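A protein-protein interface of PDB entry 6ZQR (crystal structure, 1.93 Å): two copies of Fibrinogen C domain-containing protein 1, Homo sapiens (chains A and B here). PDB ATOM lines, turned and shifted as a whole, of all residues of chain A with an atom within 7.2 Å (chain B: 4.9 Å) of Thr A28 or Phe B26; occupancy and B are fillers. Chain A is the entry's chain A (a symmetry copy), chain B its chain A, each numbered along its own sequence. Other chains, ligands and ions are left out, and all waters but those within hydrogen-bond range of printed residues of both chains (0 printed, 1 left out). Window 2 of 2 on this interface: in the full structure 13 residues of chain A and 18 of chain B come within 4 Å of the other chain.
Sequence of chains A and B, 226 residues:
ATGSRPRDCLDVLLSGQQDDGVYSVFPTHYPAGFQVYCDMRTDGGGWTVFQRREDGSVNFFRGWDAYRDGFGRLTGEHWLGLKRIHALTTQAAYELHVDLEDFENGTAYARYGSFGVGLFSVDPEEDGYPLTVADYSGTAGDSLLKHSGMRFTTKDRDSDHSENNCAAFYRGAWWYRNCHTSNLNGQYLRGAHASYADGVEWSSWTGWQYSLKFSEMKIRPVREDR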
ATOM      1  N   ARG A   5     -22.823  -3.975  -8.552  1.00  0.00           N
ATOM      2  CA  ARG A   5     -23.007  -5.300  -9.191  1.00  0.00           C
ATOM      3  C   ARG A   5     -21.772  -5.638 -10.016  1.00  0.00           C
ATOM      4  O   ARG A   5     -21.823  -5.699 -11.239  1.00  0.00           O
ATOM      5  CB  ARG A   5     -24.293  -5.297 -10.017  1.00  0.00           C
ATOM      6  CG  ARG A   5     -25.557  -5.290  -9.168  1.00  0.00           C
ATOM      7  CD  ARG A   5     -26.791  -5.204 -10.050  1.00  0.00           C
ATOM      8  NE  ARG A   5     -26.967  -6.412 -10.846  1.00  0.00           N
ATOM      9  CZ  ARG A   5     -27.465  -7.564 -10.394  1.00  0.00           C
ATOM     10  NH1 ARG A   5     -27.841  -7.691  -9.128  1.00  0.00           N
ATOM     11  NH2 ARG A   5     -27.578  -8.594 -11.212  1.00  0.00           N
ATOM     12  N   ARG A   7     -19.301  -7.901 -12.033  1.00  0.00           N
ATOM     13  CA  ARG A   7     -19.571  -9.112 -12.854  1.00  0.00           C
ATOM     14  C   ARG A   7     -18.548 -10.213 -12.533  1.00  0.00           C
ATOM     15  O   ARG A   7     -18.792 -11.374 -12.910  1.00  0.00           O
ATOM     16  CB  ARG A   7     -19.561  -8.734 -14.334  1.00  0.00           C
ATOM     17  CG  ARG A   7     -18.158  -8.648 -14.904  1.00  0.00           C
ATOM     18  CD  ARG A   7     -18.093  -7.939 -16.232  1.00  0.00           C
ATOM     19  NE  ARG A   7     -16.704  -7.760 -16.647  1.00  0.00           N
ATOM     20  CZ  ARG A   7     -16.318  -7.560 -17.904  1.00  0.00           C
ATOM     21  NH1 ARG A   7     -17.214  -7.543 -18.880  1.00  0.00           N
ATOM     22  NH2 ARG A   7     -15.038  -7.382 -18.179  1.00  0.00           N
ATOM     23  N   PHE A  26     -21.942 -10.952 -10.104  1.00  0.00           N
ATOM     24  CA  PHE A  26     -23.263 -10.960 -10.781  1.00  0.00           C
ATOM     25  C   PHE A  26     -23.026 -11.012 -12.284  1.00  0.00           C
ATOM     26  O   PHE A  26     -22.971  -9.979 -12.950  1.00  0.00           O
ATOM     27  CB  PHE A  26     -24.057  -9.721 -10.392  1.00  0.00           C
ATOM     28  CG  PHE A  26     -24.222  -9.544  -8.909  1.00  0.00           C
ATOM     29  CD1 PHE A  26     -23.249  -8.897  -8.165  1.00  0.00           C
ATOM     30  CD2 PHE A  26     -25.365  -9.993  -8.270  1.00  0.00           C
ATOM     31  CE1 PHE A  26     -23.400  -8.741  -6.794  1.00  0.00           C
ATOM     32  CE2 PHE A  26     -25.519  -9.831  -6.899  1.00  0.00           C
ATOM     33  CZ  PHE A  26     -24.532  -9.212  -6.164  1.00  0.00           C
ATOM     34  N   PRO A  27     -22.791 -12.208 -12.846  1.00  0.00           N
ATOM     35  CA  PRO A  27     -22.548 -12.319 -14.279  1.00  0.00           C
ATOM     36  C   PRO A  27     -23.784 -11.914 -15.108  1.00  0.00           C
ATOM     37  O   PRO A  27     -24.905 -11.880 -14.609  1.00  0.00           O
ATOM     38  CB  PRO A  27     -22.158 -13.789 -14.469  1.00  0.00           C
ATOM     39  CG  PRO A  27     -21.787 -14.263 -13.100  1.00  0.00           C
ATOM     40  CD  PRO A  27     -22.663 -13.489 -12.145  1.00  0.00           C
ATOM     41  N   THR A  28     -23.535 -11.542 -16.365  1.00  0.00           N
ATOM     42  CA  THR A  28     -24.557 -11.020 -17.304  1.00  0.00           C
ATOM     43  C   THR A  28     -25.815 -11.899 -17.270  1.00  0.00           C
ATOM     44  O   THR A  28     -26.927 -11.353 -17.118  1.00  0.00           O
ATOM     45  CB  THR A  28     -23.969 -10.946 -18.715  1.00  0.00           C
ATOM     46  OG1 THR A  28     -22.906  -9.997 -18.638  1.00  0.00           O
ATOM     47  CG2 THR A  28     -24.974 -10.491 -19.750  1.00  0.00           C
ATOM     48  N   HIS A  29     -25.651 -13.212 -17.440  1.00  0.00           N
ATOM     49  CA  HIS A  29     -26.767 -14.164 -17.648  1.00  0.00           C
ATOM     50  C   HIS A  29     -26.997 -14.978 -16.375  1.00  0.00           C
ATOM     51  O   HIS A  29     -27.710 -15.998 -16.439  1.00  0.00           O
ATOM     52  CB  HIS A  29     -26.507 -15.014 -18.901  1.00  0.00           C
ATOM     53  CG  HIS A  29     -26.525 -14.214 -20.160  1.00  0.00           C
ATOM     54  ND1 HIS A  29     -27.573 -13.349 -20.475  1.00  0.00           N
ATOM     55  CD2 HIS A  29     -25.625 -14.121 -21.165  1.00  0.00           C
ATOM     56  CE1 HIS A  29     -27.321 -12.784 -21.636  1.00  0.00           C
ATOM     57  NE2 HIS A  29     -26.125 -13.242 -22.080  1.00  0.00           N
ATOM     58  N   TYR A  30     -26.493 -14.498 -15.235  1.00  0.00           N
ATOM     59  CA  TYR A  30     -26.727 -15.127 -13.907  1.00  0.00           C
ATOM     60  C   TYR A  30     -26.986 -14.010 -12.907  1.00  0.00           C
ATOM     61  O   TYR A  30     -26.216 -13.834 -11.972  1.00  0.00           O
ATOM     62  CB  TYR A  30     -25.517 -15.991 -13.552  1.00  0.00           C
ATOM     63  CG  TYR A  30     -25.755 -17.121 -12.586  1.00  0.00           C
ATOM     64  CD1 TYR A  30     -26.396 -16.934 -11.367  1.00  0.00           C
ATOM     65  CD2 TYR A  30     -25.235 -18.377 -12.860  1.00  0.00           C
ATOM     66  CE1 TYR A  30     -26.556 -17.983 -10.472  1.00  0.00           C
ATOM     67  CE2 TYR A  30     -25.391 -19.435 -11.981  1.00  0.00           C
ATOM     68  CZ  TYR A  30     -26.065 -19.238 -10.790  1.00  0.00           C
ATOM     69  OH  TYR A  30     -26.179 -20.285  -9.923  1.00  0.00           O
ATOM     70  N   PRO A  31     -28.065 -13.214 -13.098  1.00  0.00           N
ATOM     71  CA  PRO A  31     -28.241 -11.958 -12.372  1.00  0.00           C
ATOM     72  C   PRO A  31     -28.515 -12.108 -10.862  1.00  0.00           C
ATOM     73  O   PRO A  31     -28.263 -11.132 -10.154  1.00  0.00           O
ATOM     74  CB  PRO A  31     -29.440 -11.287 -13.072  1.00  0.00           C
ATOM     75  CG  PRO A  31     -30.219 -12.442 -13.671  1.00  0.00           C
ATOM     76  CD  PRO A  31     -29.170 -13.484 -14.034  1.00  0.00           C
ATOM     77  N   ALA A  87     -21.200 -19.082 -16.993  1.00  0.00           N
ATOM     78  CA  ALA A  87     -21.817 -17.746 -16.810  1.00  0.00           C
ATOM     79  C   ALA A  87     -20.724 -16.675 -16.796  1.00  0.00           C
ATOM     80  O   ALA A  87     -20.950 -15.569 -17.322  1.00  0.00           O
ATOM     81  CB  ALA A  87     -22.630 -17.699 -15.536  1.00  0.00           C
ATOM     82  N   LEU A  88     -19.588 -16.973 -16.163  1.00  0.00           N
ATOM     83  CA  LEU A  88     -18.438 -16.045 -16.124  1.00  0.00           C
ATOM     84  C   LEU A  88     -17.766 -15.963 -17.501  1.00  0.00           C
ATOM     85  O   LEU A  88     -17.592 -14.834 -17.989  1.00  0.00           O
ATOM     86  CB  LEU A  88     -17.468 -16.514 -15.042  1.00  0.00           C
ATOM     87  CG  LEU A  88     -17.941 -16.238 -13.619  1.00  0.00           C
ATOM     88  CD1 LEU A  88     -17.170 -17.087 -12.626  1.00  0.00           C
ATOM     89  CD2 LEU A  88     -17.811 -14.763 -13.273  1.00  0.00           C
ATOM     90  N   THR A  90     -18.562 -16.595 -20.592  1.00  0.00           N
ATOM     91  CA  THR A  90     -19.342 -16.145 -21.778  1.00  0.00           C
ATOM     92  C   THR A  90     -19.580 -14.630 -21.763  1.00  0.00           C
ATOM     93  O   THR A  90     -20.011 -14.092 -22.816  1.00  0.00           O
ATOM     94  CB  THR A  90     -20.688 -16.864 -21.890  1.00  0.00           C
ATOM     95  OG1 THR A  90     -21.445 -16.643 -20.700  1.00  0.00           O
ATOM     96  CG2 THR A  90     -20.513 -18.342 -22.141  1.00  0.00           C
ATOM     97  N   GLN A  91     -19.343 -13.955 -20.636  1.00  0.00           N
ATOM     98  CA  GLN A  91     -19.704 -12.523 -20.477  1.00  0.00           C
ATOM     99  C   GLN A  91     -18.569 -11.618 -20.975  1.00  0.00           C
ATOM    100  O   GLN A  91     -18.851 -10.433 -21.222  1.00  0.00           O
ATOM    101  CB  GLN A  91     -20.125 -12.222 -19.035  1.00  0.00           C
ATOM    102  CG  GLN A  91     -18.981 -12.018 -18.066  1.00  0.00           C
ATOM    103  CD  GLN A  91     -19.502 -11.794 -16.668  1.00  0.00           C
ATOM    104  OE1 GLN A  91     -20.603 -11.286 -16.492  1.00  0.00           O
ATOM    105  NE2 GLN A  91     -18.692 -12.116 -15.667  1.00  0.00           N
ATOM    106  N   ALA A  92     -17.347 -12.137 -21.122  1.00  0.00           N
ATOM    107  CA  ALA A  92     -16.167 -11.397 -21.633  1.00  0.00           C
ATOM    108  C   ALA A  92     -15.096 -12.389 -22.099  1.00  0.00           C
ATOM    109  O   ALA A  92     -15.304 -13.603 -21.934  1.00  0.00           O
ATOM    110  CB  ALA A  92     -15.653 -10.477 -20.563  1.00  0.00           C
ATOM    111  N   SER B   4     -27.439  -1.441 -23.427  1.00  0.00           N
ATOM    112  CA  SER B   4     -27.418  -1.984 -22.032  1.00  0.00           C
ATOM    113  C   SER B   4     -28.098  -3.360 -22.000  1.00  0.00           C
ATOM    114  O   SER B   4     -27.386  -4.379 -21.758  1.00  0.00           O
ATOM    115  CB  SER B   4     -28.075  -1.027 -21.058  1.00  0.00           C
ATOM    116  OG  SER B   4     -28.288  -1.652 -19.800  1.00  0.00           O
ATOM    117  N   ARG B   5     -29.417  -3.372 -22.239  1.00  0.00           N
ATOM    118  CA  ARG B   5     -30.275  -4.581 -22.215  1.00  0.00           C
ATOM    119  C   ARG B   5     -31.120  -4.625 -23.482  1.00  0.00           C
ATOM    120  O   ARG B   5     -32.336  -4.481 -23.439  1.00  0.00           O
ATOM    121  CB  ARG B   5     -31.116  -4.587 -20.938  1.00  0.00           C
ATOM    122  CG  ARG B   5     -30.305  -4.874 -19.682  1.00  0.00           C
ATOM    123  CD  ARG B   5     -31.185  -4.783 -18.447  1.00  0.00           C
ATOM    124  NE  ARG B   5     -32.179  -5.849 -18.417  1.00  0.00           N
ATOM    125  CZ  ARG B   5     -31.940  -7.112 -18.059  1.00  0.00           C
ATOM    126  NH1 ARG B   5     -30.723  -7.497 -17.699  1.00  0.00           N
ATOM    127  NH2 ARG B   5     -32.924  -7.992 -18.070  1.00  0.00           N
ATOM    128  N   PRO B   6     -30.507  -4.894 -24.654  1.00  0.00           N
ATOM    129  CA  PRO B   6     -31.285  -5.092 -25.866  1.00  0.00           C
ATOM    130  C   PRO B   6     -32.206  -6.311 -25.708  1.00  0.00           C
ATOM    131  O   PRO B   6     -31.772  -7.328 -25.185  1.00  0.00           O
ATOM    132  CB  PRO B   6     -30.219  -5.316 -26.947  1.00  0.00           C
ATOM    133  CG  PRO B   6     -29.019  -5.829 -26.188  1.00  0.00           C
ATOM    134  CD  PRO B   6     -29.068  -5.105 -24.860  1.00  0.00           C
ATOM    135  N   ARG B   7     -33.440  -6.204 -26.206  1.00  0.00           N
ATOM    136  CA  ARG B   7     -34.460  -7.279 -26.083  1.00  0.00           C
ATOM    137  C   ARG B   7     -34.310  -8.291 -27.230  1.00  0.00           C
ATOM    138  O   ARG B   7     -34.884  -9.390 -27.126  1.00  0.00           O
ATOM    139  CB  ARG B   7     -35.854  -6.654 -26.048  1.00  0.00           C
ATOM    140  CG  ARG B   7     -36.371  -6.307 -27.432  1.00  0.00           C
ATOM    141  CD  ARG B   7     -37.557  -5.379 -27.413  1.00  0.00           C
ATOM    142  NE  ARG B   7     -37.907  -4.970 -28.771  1.00  0.00           N
ATOM    143  CZ  ARG B   7     -39.103  -4.514 -29.131  1.00  0.00           C
ATOM    144  NH1 ARG B   7     -40.080  -4.434 -28.240  1.00  0.00           N
ATOM    145  NH2 ARG B   7     -39.316  -4.142 -30.381  1.00  0.00           N
ATOM    146  N   SER B  24     -25.626 -11.006 -26.475  1.00  0.00           N
ATOM    147  CA  SER B  24     -26.587 -11.104 -25.347  1.00  0.00           C
ATOM    148  C   SER B  24     -27.846 -10.278 -25.648  1.00  0.00           C
ATOM    149  O   SER B  24     -27.726  -9.066 -25.977  1.00  0.00           O
ATOM    150  CB  SER B  24     -25.940 -10.659 -24.089  1.00  0.00           C
ATOM    151  OG  SER B  24     -24.902 -11.557 -23.762  1.00  0.00           O
ATOM    152  N   VAL B  25     -29.011 -10.907 -25.500  1.00  0.00           N
ATOM    153  CA  VAL B  25     -30.332 -10.233 -25.555  1.00  0.00           C
ATOM    154  C   VAL B  25     -31.106 -10.621 -24.292  1.00  0.00           C
ATOM    155  O   VAL B  25     -30.748 -11.624 -23.641  1.00  0.00           O
ATOM    156  CB  VAL B  25     -31.086 -10.565 -26.860  1.00  0.00           C
ATOM    157  CG1 VAL B  25     -30.276 -10.156 -28.088  1.00  0.00           C
ATOM    158  CG2 VAL B  25     -31.491 -12.031 -26.953  1.00  0.00           C
ATOM    159  N   PHE B  26     -32.114  -9.828 -23.946  1.00  0.00           N
ATOM    160  CA  PHE B  26     -32.811  -9.875 -22.636  1.00  0.00           C
ATOM    161  C   PHE B  26     -34.295  -9.640 -22.878  1.00  0.00           C
ATOM    162  O   PHE B  26     -34.774  -8.509 -22.810  1.00  0.00           O
ATOM    163  CB  PHE B  26     -32.233  -8.822 -21.700  1.00  0.00           C
ATOM    164  CG  PHE B  26     -30.745  -8.923 -21.514  1.00  0.00           C
ATOM    165  CD1 PHE B  26     -29.882  -8.304 -22.402  1.00  0.00           C
ATOM    166  CD2 PHE B  26     -30.217  -9.605 -20.431  1.00  0.00           C
ATOM    167  CE1 PHE B  26     -28.507  -8.404 -22.233  1.00  0.00           C
ATOM    168  CE2 PHE B  26     -28.841  -9.701 -20.259  1.00  0.00           C
ATOM    169  CZ  PHE B  26     -27.991  -9.105 -21.165  1.00  0.00           C
ATOM    170  N   PRO B  27     -35.047 -10.686 -23.255  1.00  0.00           N
ATOM    171  CA  PRO B  27     -36.472 -10.521 -23.510  1.00  0.00           C
ATOM    172  C   PRO B  27     -37.247 -10.127 -22.235  1.00  0.00           C
ATOM    173  O   PRO B  27     -36.773 -10.311 -21.117  1.00  0.00           O
ATOM    174  CB  PRO B  27     -36.902 -11.880 -24.072  1.00  0.00           C
ATOM    175  CG  PRO B  27     -35.626 -12.535 -24.496  1.00  0.00           C
ATOM    176  CD  PRO B  27     -34.572 -12.044 -23.534  1.00  0.00           C
ATOM    177  N   THR B  28     -38.417  -9.518 -22.439  1.00  0.00           N
ATOM    178  CA  THR B  28     -39.274  -8.967 -21.363  1.00  0.00           C
ATOM    179  C   THR B  28     -39.417  -9.980 -20.218  1.00  0.00           C
ATOM    180  O   THR B  28     -39.197  -9.602 -19.049  1.00  0.00           O
ATOM    181  CB  THR B  28     -40.639  -8.584 -21.939  1.00  0.00           C
ATOM    182  OG1 THR B  28     -40.380  -7.544 -22.881  1.00  0.00           O
ATOM    183  CG2 THR B  28     -41.602  -8.079 -20.888  1.00  0.00           C
ATOM    184  N   TYR B  30     -37.868 -12.950 -19.853  1.00  0.00           N
ATOM    185  CA  TYR B  30     -36.672 -13.821 -19.695  1.00  0.00           C
ATOM    186  C   TYR B  30     -35.502 -12.930 -19.304  1.00  0.00           C
ATOM    187  O   TYR B  30     -34.535 -12.828 -20.047  1.00  0.00           O
ATOM    188  CB  TYR B  30     -36.443 -14.585 -20.999  1.00  0.00           C
ATOM    189  CG  TYR B  30     -35.689 -15.884 -20.897  1.00  0.00           C
ATOM    190  CD1 TYR B  30     -34.470 -15.985 -20.237  1.00  0.00           C
ATOM    191  CD2 TYR B  30     -36.162 -17.005 -21.562  1.00  0.00           C
ATOM    192  CE1 TYR B  30     -33.771 -17.183 -20.202  1.00  0.00           C
ATOM    193  CE2 TYR B  30     -35.479 -18.208 -21.533  1.00  0.00           C
ATOM    194  CZ  TYR B  30     -34.287 -18.299 -20.839  1.00  0.00           C
ATOM    195  OH  TYR B  30     -33.613 -19.485 -20.850  1.00  0.00           O
ATOM    196  N   PRO B  31     -35.578 -12.246 -18.138  1.00  0.00           N
ATOM    197  CA  PRO B  31     -34.652 -11.162 -17.813  1.00  0.00           C
ATOM    198  C   PRO B  31     -33.197 -11.599 -17.558  1.00  0.00           C
ATOM    199  O   PRO B  31     -32.327 -10.737 -17.691  1.00  0.00           O
ATOM    200  CB  PRO B  31     -35.254 -10.526 -16.544  1.00  0.00           C
ATOM    201  CG  PRO B  31     -36.056 -11.645 -15.908  1.00  0.00           C
ATOM    202  CD  PRO B  31     -36.569 -12.478 -17.073  1.00  0.00           C
ATOM    203  N   ALA B  32     -32.943 -12.883 -17.277  1.00  0.00           N
ATOM    204  CA  ALA B  32     -31.571 -13.447 -17.190  1.00  0.00           C
ATOM    205  C   ALA B  32     -30.884 -13.271 -18.549  1.00  0.00           C
ATOM    206  O   ALA B  32     -29.673 -13.063 -18.583  1.00  0.00           O
ATOM    207  CB  ALA B  32     -31.608 -14.897 -16.796  1.00  0.00           C
ATOM    208  N   GLY B  33     -31.672 -13.308 -19.624  1.00  0.00           N
ATOM    209  CA  GLY B  33     -31.167 -13.154 -20.996  1.00  0.00           C
ATOM    210  C   GLY B  33     -30.480 -14.409 -21.472  1.00  0.00           C
ATOM    211  O   GLY B  33     -30.373 -15.399 -20.722  1.00  0.00           O
ATOM    212  N   GLN B  91     -42.946 -10.655 -26.892  1.00  0.00           N
ATOM    213  CA  GLN B  91     -42.554  -9.324 -26.362  1.00  0.00           C
ATOM    214  C   GLN B  91     -42.866  -8.220 -27.382  1.00  0.00           C
ATOM    215  O   GLN B  91     -42.914  -7.051 -26.961  1.00  0.00           O
ATOM    216  CB  GLN B  91     -41.091  -9.326 -25.907  1.00  0.00           C
ATOM    217  CG  GLN B  91     -40.077  -9.158 -27.019  1.00  0.00           C
ATOM    218  CD  GLN B  91     -38.673  -9.241 -26.473  1.00  0.00           C
ATOM    219  OE1 GLN B  91     -38.436  -8.903 -25.320  1.00  0.00           O
ATOM    220  NE2 GLN B  91     -37.724  -9.632 -27.315  1.00  0.00           N
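Printed residues of chain B within 4 Å of Thr A28: Phe B26 (3.6 Å) and Ala B32 (3.6 Å). Phe B26 touches just these residues of chain A: Thr A28 (3.6 Å) and His A29 (3.7 Å). Of the printed residues of chain B, Pro A31 touches Ala B32 (3.9 Å). Of the printed residues of chain A, Ser B24 touches His A29. Val B25 touches none of the printed residues of chain A. The nearest printed residue of chain A that does not touch Ser B24 is Thr A28 (4.2 Å).
Thr A28 touches Phe B26, but with the chains exchanged Phe A26 does not touch Thr B28 (17.3 Å). 8 positions are printed for both chains.
NE2 of His A29 lies within hydrogen-bond range of OG of Ser B24, at 2.7 Å. A ring nitrogen (ND1) of His A29 lies within hydrogen-bond range of the backbone carbonyl oxygen (O) of Ala B32 (2.8 Å). The backbone carbonyl oxygen (O) of Gly B33 sits close to a ring nitrogen (ND1) of His A29 (3.5 Å).
The backbone NH (N) of Phe B26 is in hydrogen-bond range of the backbone carbonyl oxygen (O) of Pro B6 (2.8 Å). NH2 of Arg A5 is in hydrogen-bond range of O of Pro A31 (2.8 Å). N of Thr A28 is in hydrogen-bond range of OE1 of Gln A91.
Thr A28 touches Phe B26 (CG2 to CZ, 3.6 Å). Thr A28 touches Ala B32. His A29 touches Phe B26. Pro A31 touches Ala B32 (CG to CA, 3.9 Å).
Printed residues of chain B that touch a printed residue of chain A: Ser B24, Phe B26, Ala B32 and Gly B33. Hydrophobic or aromatic side chains of chain B that line the printed part of chain A: Phe B26 and Ala B32.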
